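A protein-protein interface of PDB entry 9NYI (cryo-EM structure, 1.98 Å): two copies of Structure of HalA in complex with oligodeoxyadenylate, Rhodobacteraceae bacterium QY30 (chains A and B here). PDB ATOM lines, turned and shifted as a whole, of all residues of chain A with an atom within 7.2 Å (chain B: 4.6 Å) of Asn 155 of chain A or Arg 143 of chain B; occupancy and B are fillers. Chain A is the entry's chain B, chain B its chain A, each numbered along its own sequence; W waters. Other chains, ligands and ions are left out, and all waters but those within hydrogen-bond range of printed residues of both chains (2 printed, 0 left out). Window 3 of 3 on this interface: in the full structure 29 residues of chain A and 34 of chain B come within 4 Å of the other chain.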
ATOM      1  N   GLN A 134       3.322  12.295  22.264  1.00  0.00           N
ATOM      2  CA  GLN A 134       3.587  13.666  21.822  1.00  0.00           C
ATOM      3  C   GLN A 134       4.651  13.689  20.727  1.00  0.00           C
ATOM      4  O   GLN A 134       5.511  14.570  20.684  1.00  0.00           O
ATOM      5  CB  GLN A 134       3.984  14.562  22.999  1.00  0.00           C
ATOM      6  CG  GLN A 134       2.829  14.881  23.936  1.00  0.00           C
ATOM      7  CD  GLN A 134       3.153  15.995  24.911  1.00  0.00           C
ATOM      8  OE1 GLN A 134       3.955  15.819  25.828  1.00  0.00           O
ATOM      9  NE2 GLN A 134       2.530  17.151  24.716  1.00  0.00           N
ATOM     10  N   CYS A 135       4.587  12.706  19.833  1.00  0.00           N
ATOM     11  CA  CYS A 135       5.552  12.541  18.758  1.00  0.00           C
ATOM     12  C   CYS A 135       4.830  12.475  17.424  1.00  0.00           C
ATOM     13  O   CYS A 135       3.742  11.899  17.326  1.00  0.00           O
ATOM     14  CB  CYS A 135       6.382  11.267  18.955  1.00  0.00           C
ATOM     15  SG  CYS A 135       7.584  10.934  17.647  1.00  0.00           S
ATOM     16  N   TYR A 152       2.973   4.715  23.947  1.00  0.00           N
ATOM     17  CA  TYR A 152       2.448   5.583  22.904  1.00  0.00           C
ATOM     18  C   TYR A 152       1.088   6.110  23.339  1.00  0.00           C
ATOM     19  O   TYR A 152       0.512   5.660  24.332  1.00  0.00           O
ATOM     20  CB  TYR A 152       2.356   4.858  21.554  1.00  0.00           C
ATOM     21  CG  TYR A 152       1.790   3.454  21.619  1.00  0.00           C
ATOM     22  CD1 TYR A 152       0.552   3.204  22.199  1.00  0.00           C
ATOM     23  CD2 TYR A 152       2.487   2.381  21.081  1.00  0.00           C
ATOM     24  CE1 TYR A 152       0.035   1.927  22.257  1.00  0.00           C
ATOM     25  CE2 TYR A 152       1.973   1.101  21.127  1.00  0.00           C
ATOM     26  CZ  TYR A 152       0.748   0.879  21.719  1.00  0.00           C
ATOM     27  OH  TYR A 152       0.232  -0.396  21.771  1.00  0.00           O
ATOM     28  N   SER A 153       0.578   7.073  22.578  1.00  0.00           N
ATOM     29  CA  SER A 153      -0.715   7.685  22.845  1.00  0.00           C
ATOM     30  C   SER A 153      -1.606   7.536  21.622  1.00  0.00           C
ATOM     31  O   SER A 153      -1.148   7.688  20.488  1.00  0.00           O
ATOM     32  CB  SER A 153      -0.565   9.166  23.211  1.00  0.00           C
ATOM     33  OG  SER A 153      -1.772   9.869  22.988  1.00  0.00           O
ATOM     34  N   GLY A 154      -2.884   7.237  21.860  1.00  0.00           N
ATOM     35  CA  GLY A 154      -3.804   7.038  20.755  1.00  0.00           C
ATOM     36  C   GLY A 154      -4.007   8.278  19.906  1.00  0.00           C
ATOM     37  O   GLY A 154      -4.228   8.176  18.697  1.00  0.00           O
ATOM     38  N   ASN A 155      -3.944   9.461  20.518  1.00  0.00           N
ATOM     39  CA  ASN A 155      -4.122  10.708  19.786  1.00  0.00           C
ATOM     40  C   ASN A 155      -2.851  11.530  19.641  1.00  0.00           C
ATOM     41  O   ASN A 155      -2.734  12.284  18.674  1.00  0.00           O
ATOM     42  CB  ASN A 155      -5.198  11.576  20.455  1.00  0.00           C
ATOM     43  CG  ASN A 155      -4.804  12.031  21.846  1.00  0.00           C
ATOM     44  OD1 ASN A 155      -4.192  11.284  22.607  1.00  0.00           O
ATOM     45  ND2 ASN A 155      -5.154  13.266  22.186  1.00  0.00           N
ATOM     46  N   GLU A 156      -1.897  11.410  20.563  1.00  0.00           N
ATOM     47  CA  GLU A 156      -0.692  12.228  20.524  1.00  0.00           C
ATOM     48  C   GLU A 156       0.522  11.488  19.976  1.00  0.00           C
ATOM     49  O   GLU A 156       1.617  12.056  19.948  1.00  0.00           O
ATOM     50  CB  GLU A 156      -0.388  12.793  21.912  1.00  0.00           C
ATOM     51  CG  GLU A 156      -1.236  14.008  22.265  1.00  0.00           C
ATOM     52  CD  GLU A 156      -0.954  15.210  21.377  1.00  0.00           C
ATOM     53  OE1 GLU A 156       0.127  15.260  20.753  1.00  0.00           O
ATOM     54  OE2 GLU A 156      -1.819  16.107  21.300  1.00  0.00           O
ATOM     55  N   THR A 157       0.363  10.245  19.539  1.00  0.00           N
ATOM     56  CA  THR A 157       1.384   9.558  18.752  1.00  0.00           C
ATOM     57  C   THR A 157       0.853   9.499  17.326  1.00  0.00           C
ATOM     58  O   THR A 157       0.142   8.563  16.953  1.00  0.00           O
ATOM     59  CB  THR A 157       1.694   8.168  19.299  1.00  0.00           C
ATOM     60  OG1 THR A 157       2.207   8.279  20.631  1.00  0.00           O
ATOM     61  CG2 THR A 157       2.728   7.469  18.421  1.00  0.00           C
ATOM     62  N   GLN A 158       1.185  10.514  16.539  1.00  0.00           N
ATOM     63  CA  GLN A 158       0.706  10.614  15.171  1.00  0.00           C
ATOM     64  C   GLN A 158       1.667   9.884  14.244  1.00  0.00           C
ATOM     65  O   GLN A 158       2.878  10.128  14.278  1.00  0.00           O
ATOM     66  CB  GLN A 158       0.562  12.081  14.763  1.00  0.00           C
ATOM     67  CG  GLN A 158      -0.203  12.917  15.782  1.00  0.00           C
ATOM     68  CD  GLN A 158      -0.492  14.326  15.299  1.00  0.00           C
ATOM     69  OE1 GLN A 158      -1.249  14.527  14.350  1.00  0.00           O
ATOM     70  NE2 GLN A 158       0.110  15.310  15.957  1.00  0.00           N
ATOM     71  N   ARG A 193      -7.326   1.194  30.527  1.00  0.00           N
ATOM     72  CA  ARG A 193      -7.453   2.279  29.571  1.00  0.00           C
ATOM     73  C   ARG A 193      -6.314   2.267  28.554  1.00  0.00           C
ATOM     74  O   ARG A 193      -6.496   2.749  27.425  1.00  0.00           O
ATOM     75  CB  ARG A 193      -7.532   3.602  30.331  1.00  0.00           C
ATOM     76  CG  ARG A 193      -7.695   4.807  29.463  1.00  0.00           C
ATOM     77  CD  ARG A 193      -8.886   4.634  28.518  1.00  0.00           C
ATOM     78  NE  ARG A 193      -9.118   5.857  27.767  1.00  0.00           N
ATOM     79  CZ  ARG A 193      -8.219   6.439  26.987  1.00  0.00           C
ATOM     80  NH1 ARG A 193      -7.118   5.808  26.610  1.00  0.00           N
ATOM     81  NH2 ARG A 193      -8.468   7.653  26.508  1.00  0.00           N
ATOM     82  N   GLU A 196      -7.570   0.296  25.481  1.00  0.00           N
ATOM     83  CA  GLU A 196      -8.227   1.137  24.482  1.00  0.00           C
ATOM     84  C   GLU A 196      -7.227   2.011  23.728  1.00  0.00           C
ATOM     85  O   GLU A 196      -7.367   2.221  22.515  1.00  0.00           O
ATOM     86  CB  GLU A 196      -9.304   2.002  25.142  1.00  0.00           C
ATOM     87  CG  GLU A 196      -9.854   3.023  24.179  1.00  0.00           C
ATOM     88  CD  GLU A 196     -10.729   4.079  24.820  1.00  0.00           C
ATOM     89  OE1 GLU A 196     -11.082   3.921  26.008  1.00  0.00           O
ATOM     90  OE2 GLU A 196     -11.071   5.064  24.134  1.00  0.00           O
ATOM     91  N   THR A 197      -6.228   2.552  24.433  1.00  0.00           N
ATOM     92  CA  THR A 197      -5.193   3.332  23.751  1.00  0.00           C
ATOM     93  C   THR A 197      -4.532   2.521  22.634  1.00  0.00           C
ATOM     94  O   THR A 197      -4.379   2.997  21.496  1.00  0.00           O
ATOM     95  CB  THR A 197      -4.143   3.810  24.759  1.00  0.00           C
ATOM     96  OG1 THR A 197      -4.671   4.900  25.523  1.00  0.00           O
ATOM     97  CG2 THR A 197      -2.873   4.262  24.044  1.00  0.00           C
ATOM     98  N   THR A 200      -6.793   2.057  19.619  1.00  0.00           N
ATOM     99  CA  THR A 200      -6.875   3.240  18.765  1.00  0.00           C
ATOM    100  C   THR A 200      -5.635   3.374  17.882  1.00  0.00           C
ATOM    101  O   THR A 200      -5.738   3.606  16.663  1.00  0.00           O
ATOM    102  CB  THR A 200      -7.058   4.487  19.634  1.00  0.00           C
ATOM    103  OG1 THR A 200      -8.268   4.366  20.392  1.00  0.00           O
ATOM    104  CG2 THR A 200      -7.123   5.740  18.776  1.00  0.00           C
ATOM    105  N   ILE A 201      -4.450   3.222  18.477  1.00  0.00           N
ATOM    106  CA  ILE A 201      -3.243   3.358  17.667  1.00  0.00           C
ATOM    107  C   ILE A 201      -3.143   2.219  16.653  1.00  0.00           C
ATOM    108  O   ILE A 201      -2.591   2.399  15.561  1.00  0.00           O
ATOM    109  CB  ILE A 201      -1.987   3.462  18.556  1.00  0.00           C
ATOM    110  CG1 ILE A 201      -0.779   3.903  17.725  1.00  0.00           C
ATOM    111  CG2 ILE A 201      -1.699   2.154  19.250  1.00  0.00           C
ATOM    112  CD1 ILE A 201      -1.033   5.130  16.883  1.00  0.00           C
ATOM    113  N   ARG B 119      -4.126  21.979  14.457  1.00  0.00           N
ATOM    114  CA  ARG B 119      -3.785  21.179  15.635  1.00  0.00           C
ATOM    115  C   ARG B 119      -4.255  21.859  16.923  1.00  0.00           C
ATOM    116  O   ARG B 119      -3.514  21.980  17.901  1.00  0.00           O
ATOM    117  CB  ARG B 119      -2.281  20.884  15.674  1.00  0.00           C
ATOM    118  CG  ARG B 119      -1.873  19.754  16.611  1.00  0.00           C
ATOM    119  CD  ARG B 119      -2.567  18.452  16.262  1.00  0.00           C
ATOM    120  NE  ARG B 119      -2.311  17.423  17.263  1.00  0.00           N
ATOM    121  CZ  ARG B 119      -2.981  16.282  17.356  1.00  0.00           C
ATOM    122  NH1 ARG B 119      -3.967  15.989  16.523  1.00  0.00           N
ATOM    123  NH2 ARG B 119      -2.653  15.414  18.307  1.00  0.00           N
ATOM    124  N   LYS B 121      -6.643  21.759  20.174  1.00  0.00           N
ATOM    125  CA  LYS B 121      -7.241  20.749  21.039  1.00  0.00           C
ATOM    126  C   LYS B 121      -8.278  21.406  21.940  1.00  0.00           C
ATOM    127  O   LYS B 121      -7.939  22.262  22.763  1.00  0.00           O
ATOM    128  CB  LYS B 121      -6.173  20.043  21.875  1.00  0.00           C
ATOM    129  CG  LYS B 121      -5.271  19.119  21.075  1.00  0.00           C
ATOM    130  CD  LYS B 121      -4.163  18.530  21.937  1.00  0.00           C
ATOM    131  CE  LYS B 121      -4.708  17.522  22.937  1.00  0.00           C
ATOM    132  NZ  LYS B 121      -3.622  16.712  23.558  1.00  0.00           N
ATOM    133  N   PHE B 122      -9.535  21.005  21.778  1.00  0.00           N
ATOM    134  CA  PHE B 122     -10.617  21.404  22.673  1.00  0.00           C
ATOM    135  C   PHE B 122     -10.852  20.258  23.650  1.00  0.00           C
ATOM    136  O   PHE B 122     -11.364  19.202  23.265  1.00  0.00           O
ATOM    137  CB  PHE B 122     -11.888  21.732  21.893  1.00  0.00           C
ATOM    138  CG  PHE B 122     -11.743  22.890  20.947  1.00  0.00           C
ATOM    139  CD1 PHE B 122     -11.271  22.696  19.659  1.00  0.00           C
ATOM    140  CD2 PHE B 122     -12.093  24.170  21.341  1.00  0.00           C
ATOM    141  CE1 PHE B 122     -11.144  23.759  18.785  1.00  0.00           C
ATOM    142  CE2 PHE B 122     -11.968  25.236  20.471  1.00  0.00           C
ATOM    143  CZ  PHE B 122     -11.493  25.030  19.192  1.00  0.00           C
ATOM    144  N   SER B 123     -10.480  20.466  24.909  1.00  0.00           N
ATOM    145  CA  SER B 123     -10.545  19.429  25.935  1.00  0.00           C
ATOM    146  C   SER B 123     -11.529  19.862  27.014  1.00  0.00           C
ATOM    147  O   SER B 123     -11.263  20.814  27.757  1.00  0.00           O
ATOM    148  CB  SER B 123      -9.162  19.164  26.527  1.00  0.00           C
ATOM    149  OG  SER B 123      -8.177  19.095  25.512  1.00  0.00           O
ATOM    150  N   GLY B 124     -12.659  19.163  27.101  1.00  0.00           N
ATOM    151  CA  GLY B 124     -13.643  19.453  28.125  1.00  0.00           C
ATOM    152  C   GLY B 124     -14.369  20.768  27.962  1.00  0.00           C
ATOM    153  O   GLY B 124     -14.848  21.325  28.952  1.00  0.00           O
ATOM    154  N   GLU B 141      -8.810  18.472  17.415  1.00  0.00           N
ATOM    155  CA  GLU B 141      -9.390  17.449  18.275  1.00  0.00           C
ATOM    156  C   GLU B 141     -10.405  18.078  19.217  1.00  0.00           C
ATOM    157  O   GLU B 141     -10.114  19.086  19.867  1.00  0.00           O
ATOM    158  CB  GLU B 141      -8.304  16.723  19.079  1.00  0.00           C
ATOM    159  CG  GLU B 141      -8.823  15.968  20.288  1.00  0.00           C
ATOM    160  CD  GLU B 141      -7.759  15.112  20.942  1.00  0.00           C
ATOM    161  OE1 GLU B 141      -7.198  14.233  20.255  1.00  0.00           O
ATOM    162  OE2 GLU B 141      -7.481  15.320  22.141  1.00  0.00           O
ATOM    163  N   PHE B 142     -11.592  17.479  19.283  1.00  0.00           N
ATOM    164  CA  PHE B 142     -12.620  17.831  20.255  1.00  0.00           C
ATOM    165  C   PHE B 142     -12.856  16.616  21.139  1.00  0.00           C
ATOM    166  O   PHE B 142     -13.292  15.569  20.649  1.00  0.00           O
ATOM    167  CB  PHE B 142     -13.924  18.250  19.572  1.00  0.00           C
ATOM    168  CG  PHE B 142     -13.818  19.507  18.753  1.00  0.00           C
ATOM    169  CD1 PHE B 142     -13.182  19.500  17.522  1.00  0.00           C
ATOM    170  CD2 PHE B 142     -14.371  20.693  19.208  1.00  0.00           C
ATOM    171  CE1 PHE B 142     -13.091  20.653  16.766  1.00  0.00           C
ATOM    172  CE2 PHE B 142     -14.282  21.850  18.456  1.00  0.00           C
ATOM    173  CZ  PHE B 142     -13.641  21.831  17.234  1.00  0.00           C
ATOM    174  N   ARG B 143     -12.574  16.753  22.432  1.00  0.00           N
ATOM    175  CA  ARG B 143     -12.654  15.635  23.364  1.00  0.00           C
ATOM    176  C   ARG B 143     -13.440  16.048  24.597  1.00  0.00           C
ATOM    177  O   ARG B 143     -13.189  17.115  25.167  1.00  0.00           O
ATOM    178  CB  ARG B 143     -11.256  15.152  23.764  1.00  0.00           C
ATOM    179  CG  ARG B 143     -11.241  13.823  24.499  1.00  0.00           C
ATOM    180  CD  ARG B 143      -9.816  13.357  24.752  1.00  0.00           C
ATOM    181  NE  ARG B 143      -9.093  13.109  23.509  1.00  0.00           N
ATOM    182  CZ  ARG B 143      -9.229  12.021  22.765  1.00  0.00           C
ATOM    183  NH1 ARG B 143     -10.046  11.041  23.113  1.00  0.00           N
ATOM    184  NH2 ARG B 143      -8.523  11.911  21.643  1.00  0.00           N
ATOM    185  N   ASN B 144     -14.384  15.197  25.005  1.00  0.00           N
ATOM    186  CA  ASN B 144     -15.183  15.411  26.214  1.00  0.00           C
ATOM    187  C   ASN B 144     -15.880  16.770  26.190  1.00  0.00           C
ATOM    188  O   ASN B 144     -15.987  17.456  27.207  1.00  0.00           O
ATOM    189  CB  ASN B 144     -14.324  15.264  27.472  1.00  0.00           C
ATOM    190  CG  ASN B 144     -13.687  13.893  27.584  1.00  0.00           C
ATOM    191  OD1 ASN B 144     -14.330  12.875  27.332  1.00  0.00           O
ATOM    192  ND2 ASN B 144     -12.417  13.860  27.970  1.00  0.00           N
ATOM    193  N   CYS B 145     -16.365  17.157  25.018  1.00  0.00           N
ATOM    194  CA  CYS B 145     -16.999  18.452  24.833  1.00  0.00           C
ATOM    195  C   CYS B 145     -18.517  18.319  24.842  1.00  0.00           C
ATOM    196  O   CYS B 145     -19.080  17.272  24.512  1.00  0.00           O
ATOM    197  CB  CYS B 145     -16.536  19.102  23.525  1.00  0.00           C
ATOM    198  SG  CYS B 145     -14.778  19.529  23.488  1.00  0.00           S
ATOM    199  N   LEU B 163     -10.444  15.228  14.680  1.00  0.00           N
ATOM    200  CA  LEU B 163     -10.989  14.135  15.479  1.00  0.00           C
ATOM    201  C   LEU B 163     -12.072  14.695  16.393  1.00  0.00           C
ATOM    202  O   LEU B 163     -11.775  15.445  17.329  1.00  0.00           O
ATOM    203  CB  LEU B 163      -9.901  13.435  16.294  1.00  0.00           C
ATOM    204  CG  LEU B 163     -10.405  12.545  17.437  1.00  0.00           C
ATOM    205  CD1 LEU B 163     -11.216  11.373  16.899  1.00  0.00           C
ATOM    206  CD2 LEU B 163      -9.251  12.047  18.294  1.00  0.00           C
ATOM    207  N   ALA B 165     -14.341  13.394  19.041  1.00  0.00           N
ATOM    208  CA  ALA B 165     -14.464  12.215  19.895  1.00  0.00           C
ATOM    209  C   ALA B 165     -15.910  11.831  20.191  1.00  0.00           C
ATOM    210  O   ALA B 165     -16.174  10.664  20.497  1.00  0.00           O
ATOM    211  CB  ALA B 165     -13.708  12.433  21.206  1.00  0.00           C
ATOM    212  N   GLU B 166     -16.852  12.771  20.106  1.00  0.00           N
ATOM    213  CA  GLU B 166     -18.262  12.514  20.392  1.00  0.00           C
ATOM    214  C   GLU B 166     -19.087  12.906  19.172  1.00  0.00           C
ATOM    215  O   GLU B 166     -19.756  13.948  19.168  1.00  0.00           O
ATOM    216  CB  GLU B 166     -18.730  13.277  21.630  1.00  0.00           C
ATOM    217  CG  GLU B 166     -18.098  12.821  22.933  1.00  0.00           C
ATOM    218  CD  GLU B 166     -16.909  13.676  23.327  1.00  0.00           C
ATOM    219  OE1 GLU B 166     -17.032  14.918  23.279  1.00  0.00           O
ATOM    220  OE2 GLU B 166     -15.855  13.108  23.679  1.00  0.00           O
HETATM  221  O   HOH W   1      -4.010  13.304  14.650  1.00  0.00           O
HETATM  222  O   HOH W   2      -0.477  17.936  19.401  1.00  0.00           O
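The guanidinium group of Arg 119 of chain B is in hydrogen-bond range of the backbone carbonyl oxygen of Asn 155 of chain A, at 3.2 Å. NH2 of Arg 119 of chain B is in salt-bridge range of OE2 of Glu 156 of chain A. NE2 of Gln 158 of chain A lies close to NE of Arg 119 of chain B, 3.5 Å away. The side-chain amino group of Lys 121 of chain B is in salt-bridge range of the side-chain carboxylate of Glu 156 of chain A. The side-chain carboxylate of Glu 141 of chain B sits at hydrogen-bond distance from the side-chain amide nitrogen of Asn 155 of chain A, at 3.0 Å.
The backbone carbonyl oxygen of Glu 141 of chain B is in hydrogen-bond range of the backbone NH of Phe 122 of chain B (2.8 Å). The side-chain carboxylate (OE1) of Glu 141 of chain B lies within salt-bridge range of the guanidinium group (NH2) of Arg 143 of chain B. The side-chain sulfur (SG) of Cys 145 of chain B is in hydrogen-bond range of the backbone carbonyl oxygen (O) of Arg 143 of chain B (3.3 Å). The backbone NH (N) of Gln 134 of chain A lies within hydrogen-bond range of the backbone carbonyl oxygen (O) of Glu 156 of chain A (2.9 Å). The backbone NH (N) of Gln 158 of chain A lies within hydrogen-bond range of the backbone carbonyl oxygen (O) of Cys 135 of chain A (3.0 Å). The side-chain hydroxyl (OG) of Ser 153 of chain A sits at hydrogen-bond distance from the backbone NH (N) of Glu 156 of chain A.
Among the printed residues, pairs that only touch across the chains: Asn 155 of chain A with Arg 143 of chain B (3.5 Å).
Of the printed residues of chain A, Glu 141 of chain B touches Asn 155. Of the printed residues of chain B, Glu 156 of chain A touches Arg 119 and Lys 121. Asn 144 of chain B touches none of the printed residues of chain A. Gly 124 of chain B touches none of the printed residues of chain A. The nearest printed residue of chain A that does not touch Arg 143 of chain B is Arg 193 of chain A (5.0 Å). The nearest printed residue of chain A that does not touch Glu 141 of chain B is Glu 156 of chain A (5.8 Å).
Printed residues of chain B that touch a printed residue of chain A: Arg 119, Lys 121, Glu 141 and Arg 143. Among the printed residues, Asp or Glu carboxylates within 4 Å of a Lys or Arg side-chain nitrogen of the other chain: Glu 156 of chain A with Arg 119 of chain B (3.2 Å) and Glu 156 of chain A with Lys 121 of chain B (3.0 Å).
No position is printed for both chains.
Water W2 lies within hydrogen-bond range of the guanidinium group of Arg 119 of chain B and the side-chain carboxylate of Glu 156 of chain A. Water W1 bridges OE1 of Gln 158 of chain A (3.0 Å) and NH1 of Arg 119 of chain B (3.3 Å).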
